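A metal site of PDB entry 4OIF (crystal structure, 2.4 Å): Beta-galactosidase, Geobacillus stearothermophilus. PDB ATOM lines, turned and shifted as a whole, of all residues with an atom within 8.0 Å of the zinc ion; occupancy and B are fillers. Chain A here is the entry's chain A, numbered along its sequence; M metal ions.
Of the 23 residues printed, 4 come within 4 Å of the zinc ion.
The nearest printed residue that does not touch the zinc ion is Thr 125 (4.5 Å).
SG of Cys 168 lies close to OG1 of Thr 125 (3.1 Å).
The backbone NH (N) of Leu 167 sits close to the side-chain sulfur (SG) of Cys 165, 3.5 Å away.
N of Val 107 lies close to SG of Cys 163.
N of Thr 125 sits close to SG of Cys 123 (3.4 Å).
SG of Cys 123 sits close to N of Ser 126 (3.2 Å).
O of Val 104 sits at hydrogen-bond distance from N of Cys 123, 3.0 Å away.
The zinc ion is bound by the side-chain sulfur (SG) of Cys 168 (2.2 Å), the side-chain sulfur (SG) of Cys 165 (2.4 Å), the side-chain sulfur (SG) of Cys 163 (2.4 Å) and the side-chain sulfur (SG) of Cys 123 (2.4 Å).
The zinc ion has four donor atoms within binding distance.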
ATOM      1  N   GLU A 103      -3.071  -4.398  -5.895  1.00  0.00           N
ATOM      2  CA  GLU A 103      -1.752  -4.954  -5.654  1.00  0.00           C
ATOM      3  C   GLU A 103      -1.511  -5.227  -4.170  1.00  0.00           C
ATOM      4  O   GLU A 103      -0.531  -5.888  -3.810  1.00  0.00           O
ATOM      5  CB  GLU A 103      -0.670  -4.006  -6.181  1.00  0.00           C
ATOM      6  CG  GLU A 103      -0.432  -2.796  -5.301  1.00  0.00           C
ATOM      7  CD  GLU A 103       0.932  -2.151  -5.525  1.00  0.00           C
ATOM      8  OE1 GLU A 103       1.424  -2.133  -6.669  1.00  0.00           O
ATOM      9  OE2 GLU A 103       1.526  -1.674  -4.545  1.00  0.00           O
ATOM     10  N   VAL A 104      -2.397  -4.729  -3.320  1.00  0.00           N
ATOM     11  CA  VAL A 104      -2.223  -4.884  -1.887  1.00  0.00           C
ATOM     12  C   VAL A 104      -2.830  -6.190  -1.402  1.00  0.00           C
ATOM     13  O   VAL A 104      -2.657  -6.564  -0.240  1.00  0.00           O
ATOM     14  CB  VAL A 104      -2.882  -3.727  -1.093  1.00  0.00           C
ATOM     15  CG1 VAL A 104      -2.316  -2.383  -1.549  1.00  0.00           C
ATOM     16  CG2 VAL A 104      -4.404  -3.781  -1.239  1.00  0.00           C
ATOM     17  N   LEU A 105      -3.537  -6.879  -2.286  1.00  0.00           N
ATOM     18  CA  LEU A 105      -4.131  -8.171  -1.945  1.00  0.00           C
ATOM     19  C   LEU A 105      -3.087  -9.262  -2.136  1.00  0.00           C
ATOM     20  O   LEU A 105      -2.311  -9.221  -3.075  1.00  0.00           O
ATOM     21  CB  LEU A 105      -5.371  -8.449  -2.821  1.00  0.00           C
ATOM     22  CG  LEU A 105      -6.558  -7.512  -2.557  1.00  0.00           C
ATOM     23  CD1 LEU A 105      -7.736  -7.744  -3.503  1.00  0.00           C
ATOM     24  CD2 LEU A 105      -7.031  -7.616  -1.107  1.00  0.00           C
ATOM     25  N   ARG A 106      -3.072 -10.242  -1.233  1.00  0.00           N
ATOM     26  CA  ARG A 106      -2.069 -11.322  -1.273  1.00  0.00           C
ATOM     27  C   ARG A 106      -2.282 -12.356  -2.373  1.00  0.00           C
ATOM     28  O   ARG A 106      -3.396 -12.628  -2.807  1.00  0.00           O
ATOM     29  CB  ARG A 106      -2.035 -12.063   0.059  1.00  0.00           C
ATOM     30  CG  ARG A 106      -1.423 -11.297   1.200  1.00  0.00           C
ATOM     31  CD  ARG A 106      -1.505 -12.108   2.499  1.00  0.00           C
ATOM     32  NE  ARG A 106      -0.670 -11.541   3.559  1.00  0.00           N
ATOM     33  CZ  ARG A 106      -0.607 -12.007   4.804  1.00  0.00           C
ATOM     34  NH1 ARG A 106      -1.360 -13.055   5.156  1.00  0.00           N
ATOM     35  NH2 ARG A 106       0.195 -11.431   5.697  1.00  0.00           N
ATOM     36  N   VAL A 107      -1.177 -12.926  -2.819  1.00  0.00           N
ATOM     37  CA  VAL A 107      -1.192 -14.122  -3.619  1.00  0.00           C
ATOM     38  C   VAL A 107      -0.720 -15.245  -2.710  1.00  0.00           C
ATOM     39  O   VAL A 107       0.385 -15.157  -2.172  1.00  0.00           O
ATOM     40  CB  VAL A 107      -0.282 -13.997  -4.854  1.00  0.00           C
ATOM     41  CG1 VAL A 107      -0.221 -15.298  -5.599  1.00  0.00           C
ATOM     42  CG2 VAL A 107      -0.762 -12.873  -5.752  1.00  0.00           C
ATOM     43  N   ARG A 113      -4.624 -15.335  -6.248  1.00  0.00           N
ATOM     44  CA  ARG A 113      -4.865 -13.987  -5.753  1.00  0.00           C
ATOM     45  C   ARG A 113      -6.118 -13.974  -4.889  1.00  0.00           C
ATOM     46  O   ARG A 113      -7.181 -14.477  -5.279  1.00  0.00           O
ATOM     47  CB  ARG A 113      -5.004 -12.991  -6.902  1.00  0.00           C
ATOM     48  CG  ARG A 113      -5.244 -11.565  -6.436  1.00  0.00           C
ATOM     49  CD  ARG A 113      -3.971 -10.921  -5.895  1.00  0.00           C
ATOM     50  NE  ARG A 113      -3.016 -10.609  -6.964  1.00  0.00           N
ATOM     51  CZ  ARG A 113      -1.946  -9.844  -6.811  1.00  0.00           C
ATOM     52  NH1 ARG A 113      -1.658  -9.298  -5.638  1.00  0.00           N
ATOM     53  NH2 ARG A 113      -1.143  -9.621  -7.841  1.00  0.00           N
ATOM     54  N   HIS A 122      -2.349  -8.211   4.062  1.00  0.00           N
ATOM     55  CA  HIS A 122      -1.806  -7.382   2.993  1.00  0.00           C
ATOM     56  C   HIS A 122      -0.539  -7.984   2.393  1.00  0.00           C
ATOM     57  O   HIS A 122       0.209  -8.687   3.077  1.00  0.00           O
ATOM     58  CB  HIS A 122      -1.494  -6.000   3.532  1.00  0.00           C
ATOM     59  CG  HIS A 122      -0.449  -6.022   4.614  1.00  0.00           C
ATOM     60  ND1 HIS A 122      -0.727  -6.401   5.908  1.00  0.00           N
ATOM     61  CD2 HIS A 122       0.868  -5.720   4.569  1.00  0.00           C
ATOM     62  CE1 HIS A 122       0.374  -6.313   6.630  1.00  0.00           C
ATOM     63  NE2 HIS A 122       1.363  -5.910   5.844  1.00  0.00           N
ATOM     64  N   CYS A 123      -0.286  -7.681   1.128  1.00  0.00           N
ATOM     65  CA  CYS A 123       1.011  -7.944   0.517  1.00  0.00           C
ATOM     66  C   CYS A 123       2.083  -7.124   1.231  1.00  0.00           C
ATOM     67  O   CYS A 123       1.979  -5.898   1.294  1.00  0.00           O
ATOM     68  CB  CYS A 123       0.949  -7.620  -0.994  1.00  0.00           C
ATOM     69  SG  CYS A 123       2.573  -7.423  -1.832  1.00  0.00           S
ATOM     70  N   PHE A 124       3.114  -7.768   1.768  1.00  0.00           N
ATOM     71  CA  PHE A 124       4.082  -7.004   2.543  1.00  0.00           C
ATOM     72  C   PHE A 124       5.133  -6.301   1.640  1.00  0.00           C
ATOM     73  O   PHE A 124       5.994  -5.558   2.139  1.00  0.00           O
ATOM     74  CB  PHE A 124       4.818  -7.890   3.567  1.00  0.00           C
ATOM     75  CG  PHE A 124       5.308  -9.234   3.042  1.00  0.00           C
ATOM     76  CD1 PHE A 124       5.981  -9.299   1.852  1.00  0.00           C
ATOM     77  CD2 PHE A 124       5.253 -10.365   3.855  1.00  0.00           C
ATOM     78  CE1 PHE A 124       6.491 -10.488   1.403  1.00  0.00           C
ATOM     79  CE2 PHE A 124       5.750 -11.588   3.423  1.00  0.00           C
ATOM     80  CZ  PHE A 124       6.389 -11.637   2.159  1.00  0.00           C
ATOM     81  N   THR A 125       5.057  -6.486   0.313  1.00  0.00           N
ATOM     82  CA  THR A 125       6.022  -5.848  -0.594  1.00  0.00           C
ATOM     83  C   THR A 125       5.447  -4.583  -1.246  1.00  0.00           C
ATOM     84  O   THR A 125       6.162  -3.610  -1.458  1.00  0.00           O
ATOM     85  CB  THR A 125       6.510  -6.816  -1.706  1.00  0.00           C
ATOM     86  OG1 THR A 125       7.322  -7.863  -1.135  1.00  0.00           O
ATOM     87  CG2 THR A 125       7.355  -6.085  -2.748  1.00  0.00           C
ATOM     88  N   SER A 126       4.144  -4.609  -1.553  1.00  0.00           N
ATOM     89  CA  SER A 126       3.461  -3.492  -2.237  1.00  0.00           C
ATOM     90  C   SER A 126       3.910  -2.077  -1.812  1.00  0.00           C
ATOM     91  O   SER A 126       3.858  -1.735  -0.620  1.00  0.00           O
ATOM     92  CB  SER A 126       1.956  -3.611  -2.037  1.00  0.00           C
ATOM     93  OG  SER A 126       1.308  -2.384  -2.260  1.00  0.00           O
ATOM     94  N   GLU A 162       2.083 -14.604   4.613  1.00  0.00           N
ATOM     95  CA  GLU A 162       3.040 -14.327   3.555  1.00  0.00           C
ATOM     96  C   GLU A 162       2.340 -14.009   2.257  1.00  0.00           C
ATOM     97  O   GLU A 162       1.130 -14.183   2.120  1.00  0.00           O
ATOM     98  CB  GLU A 162       3.996 -15.510   3.395  1.00  0.00           C
ATOM     99  CG  GLU A 162       3.299 -16.867   3.363  1.00  0.00           C
ATOM    100  CD  GLU A 162       4.278 -18.017   3.548  1.00  0.00           C
ATOM    101  OE1 GLU A 162       4.841 -18.162   4.654  1.00  0.00           O
ATOM    102  OE2 GLU A 162       4.480 -18.781   2.577  1.00  0.00           O
ATOM    103  N   CYS A 163       3.102 -13.507   1.297  1.00  0.00           N
ATOM    104  CA  CYS A 163       2.583 -13.237  -0.023  1.00  0.00           C
ATOM    105  C   CYS A 163       3.571 -13.713  -1.077  1.00  0.00           C
ATOM    106  O   CYS A 163       4.785 -13.625  -0.883  1.00  0.00           O
ATOM    107  CB  CYS A 163       2.285 -11.743  -0.202  1.00  0.00           C
ATOM    108  SG  CYS A 163       1.558 -11.352  -1.811  1.00  0.00           S
ATOM    109  N   HIS A 164       3.032 -14.243  -2.180  1.00  0.00           N
ATOM    110  CA  HIS A 164       3.830 -14.891  -3.218  1.00  0.00           C
ATOM    111  C   HIS A 164       3.650 -14.240  -4.575  1.00  0.00           C
ATOM    112  O   HIS A 164       3.981 -14.835  -5.596  1.00  0.00           O
ATOM    113  CB  HIS A 164       3.454 -16.361  -3.328  1.00  0.00           C
ATOM    114  CG  HIS A 164       3.672 -17.142  -2.077  1.00  0.00           C
ATOM    115  ND1 HIS A 164       4.762 -17.974  -1.899  1.00  0.00           N
ATOM    116  CD2 HIS A 164       2.932 -17.249  -0.949  1.00  0.00           C
ATOM    117  CE1 HIS A 164       4.690 -18.537  -0.714  1.00  0.00           C
ATOM    118  NE2 HIS A 164       3.595 -18.124  -0.119  1.00  0.00           N
ATOM    119  N   CYS A 165       3.109 -13.027  -4.598  1.00  0.00           N
ATOM    120  CA  CYS A 165       2.908 -12.311  -5.844  1.00  0.00           C
ATOM    121  C   CYS A 165       4.245 -12.003  -6.513  1.00  0.00           C
ATOM    122  O   CYS A 165       5.300 -12.244  -5.917  1.00  0.00           O
ATOM    123  CB  CYS A 165       2.125 -11.011  -5.607  1.00  0.00           C
ATOM    124  SG  CYS A 165       3.052  -9.685  -4.859  1.00  0.00           S
ATOM    125  N   ASN A 166       4.205 -11.468  -7.729  1.00  0.00           N
ATOM    126  CA  ASN A 166       5.442 -11.281  -8.477  1.00  0.00           C
ATOM    127  C   ASN A 166       6.318 -10.178  -7.855  1.00  0.00           C
ATOM    128  O   ASN A 166       7.559 -10.239  -7.968  1.00  0.00           O
ATOM    129  CB  ASN A 166       5.142 -10.983  -9.941  1.00  0.00           C
ATOM    130  CG  ASN A 166       4.567 -12.191 -10.680  1.00  0.00           C
ATOM    131  OD1 ASN A 166       4.867 -13.345 -10.345  1.00  0.00           O
ATOM    132  ND2 ASN A 166       3.760 -11.930 -11.699  1.00  0.00           N
ATOM    133  N   LEU A 167       5.699  -9.237  -7.144  1.00  0.00           N
ATOM    134  CA  LEU A 167       6.433  -8.224  -6.409  1.00  0.00           C
ATOM    135  C   LEU A 167       7.285  -8.877  -5.336  1.00  0.00           C
ATOM    136  O   LEU A 167       8.486  -8.603  -5.192  1.00  0.00           O
ATOM    137  CB  LEU A 167       5.460  -7.223  -5.793  1.00  0.00           C
ATOM    138  CG  LEU A 167       4.624  -6.422  -6.786  1.00  0.00           C
ATOM    139  CD1 LEU A 167       3.938  -5.264  -6.095  1.00  0.00           C
ATOM    140  CD2 LEU A 167       5.501  -5.920  -7.916  1.00  0.00           C
ATOM    141  N   CYS A 168       6.639  -9.756  -4.588  1.00  0.00           N
ATOM    142  CA  CYS A 168       7.290 -10.530  -3.550  1.00  0.00           C
ATOM    143  C   CYS A 168       8.327 -11.513  -4.099  1.00  0.00           C
ATOM    144  O   CYS A 168       9.338 -11.773  -3.438  1.00  0.00           O
ATOM    145  CB  CYS A 168       6.231 -11.268  -2.710  1.00  0.00           C
ATOM    146  SG  CYS A 168       5.216 -10.145  -1.659  1.00  0.00           S
ATOM    147  N   GLN A 169       8.087 -12.063  -5.290  1.00  0.00           N
ATOM    148  CA  GLN A 169       9.054 -12.971  -5.906  1.00  0.00           C
ATOM    149  C   GLN A 169      10.322 -12.198  -6.208  1.00  0.00           C
ATOM    150  O   GLN A 169      11.450 -12.685  -5.961  1.00  0.00           O
ATOM    151  CB  GLN A 169       8.496 -13.598  -7.187  1.00  0.00           C
ATOM    152  CG  GLN A 169       7.230 -14.428  -7.001  1.00  0.00           C
ATOM    153  CD  GLN A 169       7.457 -15.684  -6.207  1.00  0.00           C
ATOM    154  OE1 GLN A 169       8.559 -16.226  -6.196  1.00  0.00           O
ATOM    155  NE2 GLN A 169       6.412 -16.153  -5.523  1.00  0.00           N
ATOM    156  N   ALA A 171      11.297  -9.380  -4.787  1.00  0.00           N
ATOM    157  CA  ALA A 171      11.912  -8.997  -3.526  1.00  0.00           C
ATOM    158  C   ALA A 171      12.686 -10.155  -2.856  1.00  0.00           C
ATOM    159  O   ALA A 171      13.743  -9.950  -2.253  1.00  0.00           O
ATOM    160  CB  ALA A 171      10.848  -8.438  -2.567  1.00  0.00           C
ATOM    161  N   TRP A 224      12.913 -18.956   2.591  1.00  0.00           N
ATOM    162  CA  TRP A 224      11.635 -18.275   2.388  1.00  0.00           C
ATOM    163  C   TRP A 224      11.037 -17.825   3.722  1.00  0.00           C
ATOM    164  O   TRP A 224      10.587 -16.711   3.840  1.00  0.00           O
ATOM    165  CB  TRP A 224      10.632 -19.143   1.621  1.00  0.00           C
ATOM    166  CG  TRP A 224       9.256 -18.498   1.507  1.00  0.00           C
ATOM    167  CD1 TRP A 224       8.105 -18.882   2.142  1.00  0.00           C
ATOM    168  CD2 TRP A 224       8.899 -17.360   0.717  1.00  0.00           C
ATOM    169  NE1 TRP A 224       7.059 -18.053   1.808  1.00  0.00           N
ATOM    170  CE2 TRP A 224       7.521 -17.112   0.926  1.00  0.00           C
ATOM    171  CE3 TRP A 224       9.608 -16.521  -0.148  1.00  0.00           C
ATOM    172  CZ2 TRP A 224       6.847 -16.060   0.311  1.00  0.00           C
ATOM    173  CZ3 TRP A 224       8.941 -15.484  -0.758  1.00  0.00           C
ATOM    174  CH2 TRP A 224       7.571 -15.250  -0.526  1.00  0.00           C
ATOM    175  N   PHE A 227      12.944 -14.822   4.795  1.00  0.00           N
ATOM    176  CA  PHE A 227      12.580 -13.656   4.016  1.00  0.00           C
ATOM    177  C   PHE A 227      11.232 -13.119   4.445  1.00  0.00           C
ATOM    178  O   PHE A 227      11.016 -11.928   4.419  1.00  0.00           O
ATOM    179  CB  PHE A 227      12.542 -13.956   2.515  1.00  0.00           C
ATOM    180  CG  PHE A 227      11.805 -12.914   1.722  1.00  0.00           C
ATOM    181  CD1 PHE A 227      12.412 -11.728   1.386  1.00  0.00           C
ATOM    182  CD2 PHE A 227      10.496 -13.124   1.334  1.00  0.00           C
ATOM    183  CE1 PHE A 227      11.722 -10.760   0.662  1.00  0.00           C
ATOM    184  CE2 PHE A 227       9.809 -12.163   0.620  1.00  0.00           C
ATOM    185  CZ  PHE A 227      10.424 -10.978   0.273  1.00  0.00           C
ATOM    186  N   GLN A 231      10.925  -9.315   5.503  1.00  0.00           N
ATOM    187  CA  GLN A 231      10.080  -8.436   4.747  1.00  0.00           C
ATOM    188  C   GLN A 231       8.962  -7.865   5.626  1.00  0.00           C
ATOM    189  O   GLN A 231       8.562  -6.690   5.478  1.00  0.00           O
ATOM    190  CB  GLN A 231       9.521  -9.155   3.512  1.00  0.00           C
ATOM    191  CG  GLN A 231       8.835  -8.244   2.504  1.00  0.00           C
ATOM    192  CD  GLN A 231       9.758  -7.320   1.743  1.00  0.00           C
ATOM    193  OE1 GLN A 231      10.724  -6.790   2.280  1.00  0.00           O
ATOM    194  NE2 GLN A 231       9.432  -7.106   0.470  1.00  0.00           N
HETATM  195 ZN    ZN M   1       3.194  -9.697  -2.484  1.00  0.00          ZN
